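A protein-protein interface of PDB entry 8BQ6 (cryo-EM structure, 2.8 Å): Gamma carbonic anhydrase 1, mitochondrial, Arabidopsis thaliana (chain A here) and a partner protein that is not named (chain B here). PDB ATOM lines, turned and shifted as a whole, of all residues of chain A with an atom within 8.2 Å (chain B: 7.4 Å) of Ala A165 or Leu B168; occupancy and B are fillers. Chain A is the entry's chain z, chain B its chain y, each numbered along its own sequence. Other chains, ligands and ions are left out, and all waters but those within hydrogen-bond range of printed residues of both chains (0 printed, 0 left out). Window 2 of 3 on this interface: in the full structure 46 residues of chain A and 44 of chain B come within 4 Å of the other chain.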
ATOM      1  N   GLY A 129     -34.822  -6.113   3.926  1.00  0.00           N
ATOM      2  CA  GLY A 129     -33.904  -7.147   4.352  1.00  0.00           C
ATOM      3  C   GLY A 129     -34.322  -7.813   5.649  1.00  0.00           C
ATOM      4  O   GLY A 129     -35.242  -7.381   6.342  1.00  0.00           O
ATOM      5  N   HIS A 130     -33.614  -8.902   5.948  1.00  0.00           N
ATOM      6  CA  HIS A 130     -33.906  -9.698   7.160  1.00  0.00           C
ATOM      7  C   HIS A 130     -33.786  -8.881   8.437  1.00  0.00           C
ATOM      8  O   HIS A 130     -32.758  -8.211   8.598  1.00  0.00           O
ATOM      9  CB  HIS A 130     -32.938 -10.877   7.251  1.00  0.00           C
ATOM     10  CG  HIS A 130     -32.829 -11.723   6.029  1.00  0.00           C
ATOM     11  ND1 HIS A 130     -33.775 -12.667   5.699  1.00  0.00           N
ATOM     12  CD2 HIS A 130     -31.861 -11.815   5.095  1.00  0.00           C
ATOM     13  CE1 HIS A 130     -33.410 -13.284   4.597  1.00  0.00           C
ATOM     14  NE2 HIS A 130     -32.240 -12.778   4.205  1.00  0.00           N
ATOM     15  N   PHE A 144     -34.205  -0.329  -1.862  1.00  0.00           N
ATOM     16  CA  PHE A 144     -33.523  -1.406  -1.162  1.00  0.00           C
ATOM     17  C   PHE A 144     -33.332  -0.984   0.282  1.00  0.00           C
ATOM     18  O   PHE A 144     -32.672   0.022   0.558  1.00  0.00           O
ATOM     19  CB  PHE A 144     -32.178  -1.714  -1.821  1.00  0.00           C
ATOM     20  CG  PHE A 144     -31.532  -2.983  -1.346  1.00  0.00           C
ATOM     21  CD1 PHE A 144     -31.821  -4.190  -1.952  1.00  0.00           C
ATOM     22  CD2 PHE A 144     -30.599  -2.959  -0.324  1.00  0.00           C
ATOM     23  CE1 PHE A 144     -31.216  -5.352  -1.534  1.00  0.00           C
ATOM     24  CE2 PHE A 144     -29.988  -4.120   0.096  1.00  0.00           C
ATOM     25  CZ  PHE A 144     -30.296  -5.317  -0.513  1.00  0.00           C
ATOM     26  N   ILE A 145     -33.927  -1.737   1.194  1.00  0.00           N
ATOM     27  CA  ILE A 145     -33.748  -1.520   2.617  1.00  0.00           C
ATOM     28  C   ILE A 145     -32.814  -2.608   3.096  1.00  0.00           C
ATOM     29  O   ILE A 145     -33.138  -3.801   3.027  1.00  0.00           O
ATOM     30  CB  ILE A 145     -35.071  -1.543   3.385  1.00  0.00           C
ATOM     31  CG1 ILE A 145     -35.982  -0.436   2.870  1.00  0.00           C
ATOM     32  CG2 ILE A 145     -34.817  -1.378   4.879  1.00  0.00           C
ATOM     33  CD1 ILE A 145     -35.390   0.930   2.975  1.00  0.00           C
ATOM     34  N   GLY A 146     -31.639  -2.192   3.546  1.00  0.00           N
ATOM     35  CA  GLY A 146     -30.690  -3.131   4.077  1.00  0.00           C
ATOM     36  C   GLY A 146     -31.232  -3.852   5.292  1.00  0.00           C
ATOM     37  O   GLY A 146     -32.012  -3.319   6.083  1.00  0.00           O
ATOM     38  N   MET A 147     -30.810  -5.100   5.401  1.00  0.00           N
ATOM     39  CA  MET A 147     -31.121  -5.976   6.511  1.00  0.00           C
ATOM     40  C   MET A 147     -30.570  -5.416   7.825  1.00  0.00           C
ATOM     41  O   MET A 147     -29.526  -4.763   7.861  1.00  0.00           O
ATOM     42  CB  MET A 147     -30.609  -7.369   6.111  1.00  0.00           C
ATOM     43  CG  MET A 147     -29.125  -7.566   6.193  1.00  0.00           C
ATOM     44  SD  MET A 147     -28.536  -7.779   7.832  1.00  0.00           S
ATOM     45  CE  MET A 147     -28.766  -9.489   7.857  1.00  0.00           C
ATOM     46  N   GLY A 148     -31.344  -5.590   8.898  1.00  0.00           N
ATOM     47  CA  GLY A 148     -31.010  -5.041  10.201  1.00  0.00           C
ATOM     48  C   GLY A 148     -31.146  -3.539  10.342  1.00  0.00           C
ATOM     49  O   GLY A 148     -30.793  -3.001  11.398  1.00  0.00           O
ATOM     50  N   ALA A 149     -31.640  -2.844   9.321  1.00  0.00           N
ATOM     51  CA  ALA A 149     -31.769  -1.397   9.348  1.00  0.00           C
ATOM     52  C   ALA A 149     -33.086  -0.982   9.995  1.00  0.00           C
ATOM     53  O   ALA A 149     -34.066  -1.730  10.007  1.00  0.00           O
ATOM     54  CB  ALA A 149     -31.684  -0.826   7.934  1.00  0.00           C
ATOM     55  N   THR A 150     -33.105   0.236  10.529  1.00  0.00           N
ATOM     56  CA  THR A 150     -34.295   0.785  11.165  1.00  0.00           C
ATOM     57  C   THR A 150     -34.673   2.094  10.491  1.00  0.00           C
ATOM     58  O   THR A 150     -33.827   2.977  10.322  1.00  0.00           O
ATOM     59  CB  THR A 150     -34.079   1.009  12.668  1.00  0.00           C
ATOM     60  OG1 THR A 150     -33.728  -0.231  13.296  1.00  0.00           O
ATOM     61  CG2 THR A 150     -35.339   1.558  13.321  1.00  0.00           C
ATOM     62  N   MET A 162     -31.217   3.511  -1.408  1.00  0.00           N
ATOM     63  CA  MET A 162     -30.664   2.355  -0.723  1.00  0.00           C
ATOM     64  C   MET A 162     -30.311   2.721   0.710  1.00  0.00           C
ATOM     65  O   MET A 162     -29.631   3.720   0.962  1.00  0.00           O
ATOM     66  CB  MET A 162     -29.430   1.811  -1.451  1.00  0.00           C
ATOM     67  CG  MET A 162     -28.662   0.779  -0.658  1.00  0.00           C
ATOM     68  SD  MET A 162     -27.933  -0.535  -1.648  1.00  0.00           S
ATOM     69  CE  MET A 162     -26.323  -0.649  -0.877  1.00  0.00           C
ATOM     70  N   VAL A 163     -30.793   1.908   1.645  1.00  0.00           N
ATOM     71  CA  VAL A 163     -30.462   2.024   3.059  1.00  0.00           C
ATOM     72  C   VAL A 163     -29.544   0.859   3.393  1.00  0.00           C
ATOM     73  O   VAL A 163     -29.921  -0.304   3.211  1.00  0.00           O
ATOM     74  CB  VAL A 163     -31.723   2.011   3.935  1.00  0.00           C
ATOM     75  CG1 VAL A 163     -31.354   2.146   5.399  1.00  0.00           C
ATOM     76  CG2 VAL A 163     -32.672   3.114   3.505  1.00  0.00           C
ATOM     77  N   ALA A 164     -28.339   1.166   3.861  1.00  0.00           N
ATOM     78  CA  ALA A 164     -27.348   0.124   4.081  1.00  0.00           C
ATOM     79  C   ALA A 164     -27.742  -0.770   5.251  1.00  0.00           C
ATOM     80  O   ALA A 164     -28.523  -0.393   6.127  1.00  0.00           O
ATOM     81  CB  ALA A 164     -25.971   0.734   4.335  1.00  0.00           C
ATOM     82  N   ALA A 165     -27.187  -1.978   5.248  1.00  0.00           N
ATOM     83  CA  ALA A 165     -27.445  -2.917   6.327  1.00  0.00           C
ATOM     84  C   ALA A 165     -26.987  -2.338   7.659  1.00  0.00           C
ATOM     85  O   ALA A 165     -25.895  -1.775   7.770  1.00  0.00           O
ATOM     86  CB  ALA A 165     -26.736  -4.242   6.053  1.00  0.00           C
ATOM     87  N   GLY A 166     -27.842  -2.467   8.673  1.00  0.00           N
ATOM     88  CA  GLY A 166     -27.531  -1.972   9.998  1.00  0.00           C
ATOM     89  C   GLY A 166     -27.680  -0.480  10.195  1.00  0.00           C
ATOM     90  O   GLY A 166     -27.293   0.027  11.249  1.00  0.00           O
ATOM     91  N   ALA A 167     -28.225   0.239   9.218  1.00  0.00           N
ATOM     92  CA  ALA A 167     -28.346   1.688   9.295  1.00  0.00           C
ATOM     93  C   ALA A 167     -29.493   2.096  10.217  1.00  0.00           C
ATOM     94  O   ALA A 167     -30.426   1.332  10.468  1.00  0.00           O
ATOM     95  CB  ALA A 167     -28.565   2.280   7.905  1.00  0.00           C
ATOM     96  N   LEU A 168     -29.413   3.330  10.719  1.00  0.00           N
ATOM     97  CA  LEU A 168     -30.440   3.917  11.584  1.00  0.00           C
ATOM     98  C   LEU A 168     -30.844   5.240  10.948  1.00  0.00           C
ATOM     99  O   LEU A 168     -30.177   6.262  11.136  1.00  0.00           O
ATOM    100  CB  LEU A 168     -29.933   4.105  13.016  1.00  0.00           C
ATOM    101  CG  LEU A 168     -30.891   4.293  14.207  1.00  0.00           C
ATOM    102  CD1 LEU A 168     -31.774   5.544  14.094  1.00  0.00           C
ATOM    103  CD2 LEU A 168     -31.739   3.052  14.464  1.00  0.00           C
ATOM    104  N   VAL A 180     -26.815   5.920  -1.415  1.00  0.00           N
ATOM    105  CA  VAL A 180     -26.619   4.887  -0.406  1.00  0.00           C
ATOM    106  C   VAL A 180     -26.334   5.595   0.914  1.00  0.00           C
ATOM    107  O   VAL A 180     -25.319   6.290   1.041  1.00  0.00           O
ATOM    108  CB  VAL A 180     -25.470   3.939  -0.795  1.00  0.00           C
ATOM    109  CG1 VAL A 180     -24.958   3.166   0.410  1.00  0.00           C
ATOM    110  CG2 VAL A 180     -25.891   2.998  -1.927  1.00  0.00           C
ATOM    111  N   TRP A 181     -27.231   5.443   1.888  1.00  0.00           N
ATOM    112  CA  TRP A 181     -27.049   6.005   3.223  1.00  0.00           C
ATOM    113  C   TRP A 181     -26.855   4.879   4.226  1.00  0.00           C
ATOM    114  O   TRP A 181     -27.483   3.822   4.114  1.00  0.00           O
ATOM    115  CB  TRP A 181     -28.242   6.863   3.663  1.00  0.00           C
ATOM    116  CG  TRP A 181     -28.388   8.156   2.936  1.00  0.00           C
ATOM    117  CD1 TRP A 181     -28.241   8.357   1.600  1.00  0.00           C
ATOM    118  CD2 TRP A 181     -28.748   9.428   3.497  1.00  0.00           C
ATOM    119  NE1 TRP A 181     -28.470   9.673   1.290  1.00  0.00           N
ATOM    120  CE2 TRP A 181     -28.783  10.352   2.438  1.00  0.00           C
ATOM    121  CE3 TRP A 181     -29.034   9.874   4.791  1.00  0.00           C
ATOM    122  CZ2 TRP A 181     -29.091  11.694   2.628  1.00  0.00           C
ATOM    123  CZ3 TRP A 181     -29.345  11.206   4.976  1.00  0.00           C
ATOM    124  CH2 TRP A 181     -29.369  12.100   3.902  1.00  0.00           C
ATOM    125  N   GLY A 182     -25.997   5.115   5.218  1.00  0.00           N
ATOM    126  CA  GLY A 182     -25.701   4.082   6.189  1.00  0.00           C
ATOM    127  C   GLY A 182     -25.116   4.635   7.470  1.00  0.00           C
ATOM    128  O   GLY A 182     -24.686   5.789   7.545  1.00  0.00           O
ATOM    129  N   GLY A 183     -25.105   3.775   8.484  1.00  0.00           N
ATOM    130  CA  GLY A 183     -24.580   4.125   9.786  1.00  0.00           C
ATOM    131  C   GLY A 183     -25.650   4.612  10.738  1.00  0.00           C
ATOM    132  O   GLY A 183     -26.822   4.786  10.396  1.00  0.00           O
ATOM    133  N   ASN A 184     -25.225   4.828  11.978  1.00  0.00           N
ATOM    134  CA  ASN A 184     -26.087   5.361  13.030  1.00  0.00           C
ATOM    135  C   ASN A 184     -25.470   6.654  13.538  1.00  0.00           C
ATOM    136  O   ASN A 184     -24.413   6.621  14.193  1.00  0.00           O
ATOM    137  CB  ASN A 184     -26.242   4.346  14.163  1.00  0.00           C
ATOM    138  CG  ASN A 184     -27.215   4.794  15.236  1.00  0.00           C
ATOM    139  OD1 ASN A 184     -27.800   5.875  15.158  1.00  0.00           O
ATOM    140  ND2 ASN A 184     -27.402   3.951  16.245  1.00  0.00           N
ATOM    141  N   LEU A 189     -23.431   7.913   2.052  1.00  0.00           N
ATOM    142  CA  LEU A 189     -22.170   7.216   1.824  1.00  0.00           C
ATOM    143  C   LEU A 189     -21.643   7.406   0.412  1.00  0.00           C
ATOM    144  O   LEU A 189     -20.480   7.779   0.233  1.00  0.00           O
ATOM    145  CB  LEU A 189     -22.315   5.716   2.118  1.00  0.00           C
ATOM    146  CG  LEU A 189     -22.876   5.310   3.480  1.00  0.00           C
ATOM    147  CD1 LEU A 189     -23.105   3.807   3.532  1.00  0.00           C
ATOM    148  CD2 LEU A 189     -21.942   5.754   4.587  1.00  0.00           C
ATOM    149  N   GLY B 148     -27.799  -9.638  18.746  1.00  0.00           N
ATOM    150  CA  GLY B 148     -28.091  -8.483  17.929  1.00  0.00           C
ATOM    151  C   GLY B 148     -27.040  -8.148  16.898  1.00  0.00           C
ATOM    152  O   GLY B 148     -27.177  -7.136  16.206  1.00  0.00           O
ATOM    153  N   ALA B 149     -25.996  -8.961  16.774  1.00  0.00           N
ATOM    154  CA  ALA B 149     -24.928  -8.697  15.821  1.00  0.00           C
ATOM    155  C   ALA B 149     -25.321  -9.184  14.429  1.00  0.00           C
ATOM    156  O   ALA B 149     -26.189 -10.045  14.273  1.00  0.00           O
ATOM    157  CB  ALA B 149     -23.633  -9.371  16.275  1.00  0.00           C
ATOM    158  N   THR B 150     -24.675  -8.618  13.412  1.00  0.00           N
ATOM    159  CA  THR B 150     -25.019  -8.883  12.019  1.00  0.00           C
ATOM    160  C   THR B 150     -23.766  -9.157  11.205  1.00  0.00           C
ATOM    161  O   THR B 150     -22.914  -8.276  11.053  1.00  0.00           O
ATOM    162  CB  THR B 150     -25.785  -7.709  11.416  1.00  0.00           C
ATOM    163  OG1 THR B 150     -26.919  -7.401  12.234  1.00  0.00           O
ATOM    164  CG2 THR B 150     -26.221  -8.031  10.025  1.00  0.00           C
ATOM    165  N   LEU B 151     -23.674 -10.368  10.661  1.00  0.00           N
ATOM    166  CA  LEU B 151     -22.581 -10.777   9.792  1.00  0.00           C
ATOM    167  C   LEU B 151     -23.089 -10.816   8.359  1.00  0.00           C
ATOM    168  O   LEU B 151     -24.052 -11.531   8.058  1.00  0.00           O
ATOM    169  CB  LEU B 151     -22.044 -12.149  10.190  1.00  0.00           C
ATOM    170  CG  LEU B 151     -21.735 -12.438  11.655  1.00  0.00           C
ATOM    171  CD1 LEU B 151     -21.044 -13.773  11.741  1.00  0.00           C
ATOM    172  CD2 LEU B 151     -20.875 -11.364  12.270  1.00  0.00           C
ATOM    173  N   LEU B 152     -22.436 -10.066   7.482  1.00  0.00           N
ATOM    174  CA  LEU B 152     -22.811 -10.009   6.082  1.00  0.00           C
ATOM    175  C   LEU B 152     -22.066 -11.098   5.309  1.00  0.00           C
ATOM    176  O   LEU B 152     -21.284 -11.868   5.870  1.00  0.00           O
ATOM    177  CB  LEU B 152     -22.540  -8.610   5.533  1.00  0.00           C
ATOM    178  CG  LEU B 152     -23.351  -7.491   6.197  1.00  0.00           C
ATOM    179  CD1 LEU B 152     -23.448  -6.276   5.299  1.00  0.00           C
ATOM    180  CD2 LEU B 152     -24.740  -7.980   6.556  1.00  0.00           C
ATOM    181  N   VAL B 155     -18.083 -12.836   5.419  1.00  0.00           N
ATOM    182  CA  VAL B 155     -17.425 -12.610   6.697  1.00  0.00           C
ATOM    183  C   VAL B 155     -16.881 -13.927   7.230  1.00  0.00           C
ATOM    184  O   VAL B 155     -17.521 -14.980   7.112  1.00  0.00           O
ATOM    185  CB  VAL B 155     -18.417 -11.967   7.681  1.00  0.00           C
ATOM    186  CG1 VAL B 155     -17.911 -12.049   9.112  1.00  0.00           C
ATOM    187  CG2 VAL B 155     -18.690 -10.537   7.278  1.00  0.00           C
ATOM    188  N   VAL B 163     -17.443 -11.326  18.175  1.00  0.00           N
ATOM    189  CA  VAL B 163     -18.110 -10.172  17.590  1.00  0.00           C
ATOM    190  C   VAL B 163     -19.012  -9.600  18.672  1.00  0.00           C
ATOM    191  O   VAL B 163     -19.854 -10.316  19.227  1.00  0.00           O
ATOM    192  CB  VAL B 163     -18.919 -10.542  16.339  1.00  0.00           C
ATOM    193  CG1 VAL B 163     -19.828  -9.393  15.946  1.00  0.00           C
ATOM    194  CG2 VAL B 163     -18.001 -10.916  15.193  1.00  0.00           C
ATOM    195  N   ALA B 164     -18.834  -8.318  18.977  1.00  0.00           N
ATOM    196  CA  ALA B 164     -19.562  -7.701  20.073  1.00  0.00           C
ATOM    197  C   ALA B 164     -21.053  -7.617  19.756  1.00  0.00           C
ATOM    198  O   ALA B 164     -21.472  -7.586  18.596  1.00  0.00           O
ATOM    199  CB  ALA B 164     -19.006  -6.307  20.365  1.00  0.00           C
ATOM    200  N   ALA B 165     -21.857  -7.587  20.816  1.00  0.00           N
ATOM    201  CA  ALA B 165     -23.302  -7.500  20.660  1.00  0.00           C
ATOM    202  C   ALA B 165     -23.688  -6.218  19.934  1.00  0.00           C
ATOM    203  O   ALA B 165     -23.178  -5.136  20.239  1.00  0.00           O
ATOM    204  CB  ALA B 165     -23.981  -7.562  22.028  1.00  0.00           C
ATOM    205  N   GLY B 166     -24.591  -6.347  18.965  1.00  0.00           N
ATOM    206  CA  GLY B 166     -25.089  -5.211  18.222  1.00  0.00           C
ATOM    207  C   GLY B 166     -24.215  -4.741  17.084  1.00  0.00           C
ATOM    208  O   GLY B 166     -24.490  -3.678  16.516  1.00  0.00           O
ATOM    209  N   SER B 167     -23.178  -5.491  16.726  1.00  0.00           N
ATOM    210  CA  SER B 167     -22.248  -5.037  15.705  1.00  0.00           C
ATOM    211  C   SER B 167     -22.812  -5.250  14.308  1.00  0.00           C
ATOM    212  O   SER B 167     -23.694  -6.082  14.084  1.00  0.00           O
ATOM    213  CB  SER B 167     -20.913  -5.764  15.836  1.00  0.00           C
ATOM    214  OG  SER B 167     -20.453  -5.730  17.171  1.00  0.00           O
ATOM    215  N   LEU B 168     -22.291  -4.479  13.365  1.00  0.00           N
ATOM    216  CA  LEU B 168     -22.570  -4.661  11.947  1.00  0.00           C
ATOM    217  C   LEU B 168     -21.239  -4.956  11.274  1.00  0.00           C
ATOM    218  O   LEU B 168     -20.422  -4.051  11.077  1.00  0.00           O
ATOM    219  CB  LEU B 168     -23.242  -3.426  11.354  1.00  0.00           C
ATOM    220  CG  LEU B 168     -23.851  -3.531   9.950  1.00  0.00           C
ATOM    221  CD1 LEU B 168     -22.808  -3.350   8.862  1.00  0.00           C
ATOM    222  CD2 LEU B 168     -24.562  -4.849   9.773  1.00  0.00           C
ATOM    223  N   VAL B 169     -21.020  -6.219  10.935  1.00  0.00           N
ATOM    224  CA  VAL B 169     -19.786  -6.661  10.303  1.00  0.00           C
ATOM    225  C   VAL B 169     -19.992  -6.590   8.797  1.00  0.00           C
ATOM    226  O   VAL B 169     -20.805  -7.332   8.235  1.00  0.00           O
ATOM    227  CB  VAL B 169     -19.398  -8.073  10.755  1.00  0.00           C
ATOM    228  CG1 VAL B 169     -18.050  -8.457  10.185  1.00  0.00           C
ATOM    229  CG2 VAL B 169     -19.376  -8.140  12.272  1.00  0.00           C
ATOM    230  N   LYS B 170     -19.247  -5.705   8.142  1.00  0.00           N
ATOM    231  CA  LYS B 170     -19.415  -5.479   6.717  1.00  0.00           C
ATOM    232  C   LYS B 170     -18.952  -6.689   5.917  1.00  0.00           C
ATOM    233  O   LYS B 170     -18.289  -7.593   6.428  1.00  0.00           O
ATOM    234  CB  LYS B 170     -18.638  -4.243   6.274  1.00  0.00           C
ATOM    235  CG  LYS B 170     -19.056  -2.981   6.990  1.00  0.00           C
ATOM    236  CD  LYS B 170     -20.313  -2.400   6.377  1.00  0.00           C
ATOM    237  CE  LYS B 170     -20.046  -1.855   4.985  1.00  0.00           C
ATOM    238  NZ  LYS B 170     -18.663  -1.325   4.845  1.00  0.00           N
ATOM    239  N   GLN B 171     -19.303  -6.680   4.635  1.00  0.00           N
ATOM    240  CA  GLN B 171     -19.003  -7.795   3.750  1.00  0.00           C
ATOM    241  C   GLN B 171     -17.503  -8.047   3.671  1.00  0.00           C
ATOM    242  O   GLN B 171     -16.700  -7.111   3.635  1.00  0.00           O
ATOM    243  CB  GLN B 171     -19.554  -7.510   2.356  1.00  0.00           C
ATOM    244  CG  GLN B 171     -20.717  -8.384   1.963  1.00  0.00           C
ATOM    245  CD  GLN B 171     -21.145  -8.170   0.533  1.00  0.00           C
ATOM    246  OE1 GLN B 171     -20.424  -8.517  -0.401  1.00  0.00           O
ATOM    247  NE2 GLN B 171     -22.331  -7.603   0.352  1.00  0.00           N
ATOM    248  N   THR B 173     -15.381  -9.019   5.745  1.00  0.00           N
ATOM    249  CA  THR B 173     -14.541  -8.693   6.887  1.00  0.00           C
ATOM    250  C   THR B 173     -14.104  -9.960   7.607  1.00  0.00           C
ATOM    251  O   THR B 173     -14.894 -10.885   7.813  1.00  0.00           O
ATOM    252  CB  THR B 173     -15.287  -7.774   7.851  1.00  0.00           C
ATOM    253  OG1 THR B 173     -15.704  -6.594   7.156  1.00  0.00           O
ATOM    254  CG2 THR B 173     -14.399  -7.382   9.016  1.00  0.00           C
ATOM    255  N   GLY B 182     -16.368  -4.789  17.182  1.00  0.00           N
ATOM    256  CA  GLY B 182     -17.696  -4.287  17.479  1.00  0.00           C
ATOM    257  C   GLY B 182     -17.905  -2.920  16.873  1.00  0.00           C
ATOM    258  O   GLY B 182     -16.993  -2.319  16.301  1.00  0.00           O
ATOM    259  N   GLY B 183     -19.133  -2.430  17.015  1.00  0.00           N
ATOM    260  CA  GLY B 183     -19.528  -1.141  16.480  1.00  0.00           C
ATOM    261  C   GLY B 183     -20.201  -1.267  15.127  1.00  0.00           C
ATOM    262  O   GLY B 183     -20.386  -2.357  14.576  1.00  0.00           O
ATOM    263  N   ASN B 184     -20.574  -0.109  14.587  1.00  0.00           N
ATOM    264  CA  ASN B 184     -21.234  -0.018  13.286  1.00  0.00           C
ATOM    265  C   ASN B 184     -20.561   1.081  12.471  1.00  0.00           C
ATOM    266  O   ASN B 184     -20.851   2.272  12.672  1.00  0.00           O
ATOM    267  CB  ASN B 184     -22.725   0.263  13.440  1.00  0.00           C
ATOM    268  CG  ASN B 184     -23.497   0.039  12.159  1.00  0.00           C
ATOM    269  OD1 ASN B 184     -22.916  -0.203  11.102  1.00  0.00           O
ATOM    270  ND2 ASN B 184     -24.815   0.145  12.240  1.00  0.00           N
ATOM    271  N   PRO B 185     -19.675   0.728  11.531  1.00  0.00           N
ATOM    272  CA  PRO B 185     -19.258  -0.620  11.121  1.00  0.00           C
ATOM    273  C   PRO B 185     -18.350  -1.278  12.150  1.00  0.00           C
ATOM    274  O   PRO B 185     -17.741  -0.601  12.970  1.00  0.00           O
ATOM    275  CB  PRO B 185     -18.542  -0.362   9.789  1.00  0.00           C
ATOM    276  CG  PRO B 185     -17.980   1.012   9.938  1.00  0.00           C
ATOM    277  CD  PRO B 185     -19.014   1.770  10.725  1.00  0.00           C
ATOM    278  N   ALA B 186     -18.266  -2.605  12.143  1.00  0.00           N
ATOM    279  CA  ALA B 186     -17.480  -3.306  13.147  1.00  0.00           C
ATOM    280  C   ALA B 186     -15.995  -3.067  12.924  1.00  0.00           C
ATOM    281  O   ALA B 186     -15.507  -3.100  11.790  1.00  0.00           O
ATOM    282  CB  ALA B 186     -17.783  -4.802  13.113  1.00  0.00           C
ATOM    283  N   LYS B 187     -15.275  -2.827  14.015  1.00  0.00           N
ATOM    284  CA  LYS B 187     -13.842  -2.597  13.948  1.00  0.00           C
ATOM    285  C   LYS B 187     -13.199  -3.162  15.204  1.00  0.00           C
ATOM    286  O   LYS B 187     -13.876  -3.472  16.187  1.00  0.00           O
ATOM    287  CB  LYS B 187     -13.515  -1.107  13.785  1.00  0.00           C
ATOM    288  CG  LYS B 187     -13.854  -0.259  14.998  1.00  0.00           C
ATOM    289  CD  LYS B 187     -13.515   1.204  14.763  1.00  0.00           C
ATOM    290  CE  LYS B 187     -14.581   2.120  15.344  1.00  0.00           C
ATOM    291  NZ  LYS B 187     -14.331   2.465  16.770  1.00  0.00           N
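The backbone carbonyl oxygen of Ser B167 sits at hydrogen-bond distance from the backbone NH of Thr B150, 2.8 Å away.
O of Thr B150 is in hydrogen-bond range of N of Val B169 (2.8 Å).
The backbone carbonyl oxygen of Val B169 lies close to the backbone NH of Leu B152, at 3.3 Å.
The backbone NH (N) of Leu B168 lies within hydrogen-bond range of the backbone carbonyl oxygen (O) of Gly B183, at 3.1 Å.
The backbone carbonyl oxygen (O) of Leu B168 lies within hydrogen-bond range of the backbone NH (N) of Ala B186 (2.8 Å).
The backbone carbonyl oxygen (O) of Met A147 sits at hydrogen-bond distance from the backbone NH (N) of Gly A166.
Of the 22 printed residues of chain A, 3 touch a printed residue of chain B.
Hydrophobic or aromatic side chains of chain A that line the printed part of chain B: Met A147 and Ala A165.
Among the printed residues, 5 pairs touch across the chains.
Among the printed residues, no Asp or Glu carboxylate lies within 4 Å of a Lys or Arg side-chain nitrogen of the other chain.
Gly A129 touches none of the printed residues of chain B.
Printed residues of chain B within 4 Å of Met A147: Thr B150.
Ala A165 touches two residues of chain B.
Of the printed residues of chain B, Gly A166 touches Leu B168 (3.997 Å) and Asn B184 (2.7 Å).
Leu A189 touches none of the printed residues of chain B.
Printed residues of chain A within 4 Å of Leu B168: Ala A165 (3.5 Å) and Gly A166 (3.997 Å).
The nearest residue of chain B that does not touch Ala A165 is Asn B184 (4.7 Å).
The nearest printed residue of chain A that does not touch Asn B184 is Ala A167 (4.6 Å).
Among the printed residues, pairs that only touch across the chains: Met A147 with Thr B150 (3.2 Å), Ala A165 with Leu B168 (3.5 Å), Ala A165 with Leu B152 (3.9 Å) and Gly A166 with Leu B168 (3.997 Å).
The backbone carbonyl oxygen of Gly A166 sits at hydrogen-bond distance from the side-chain amide nitrogen of Asn B184 (2.7 Å).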
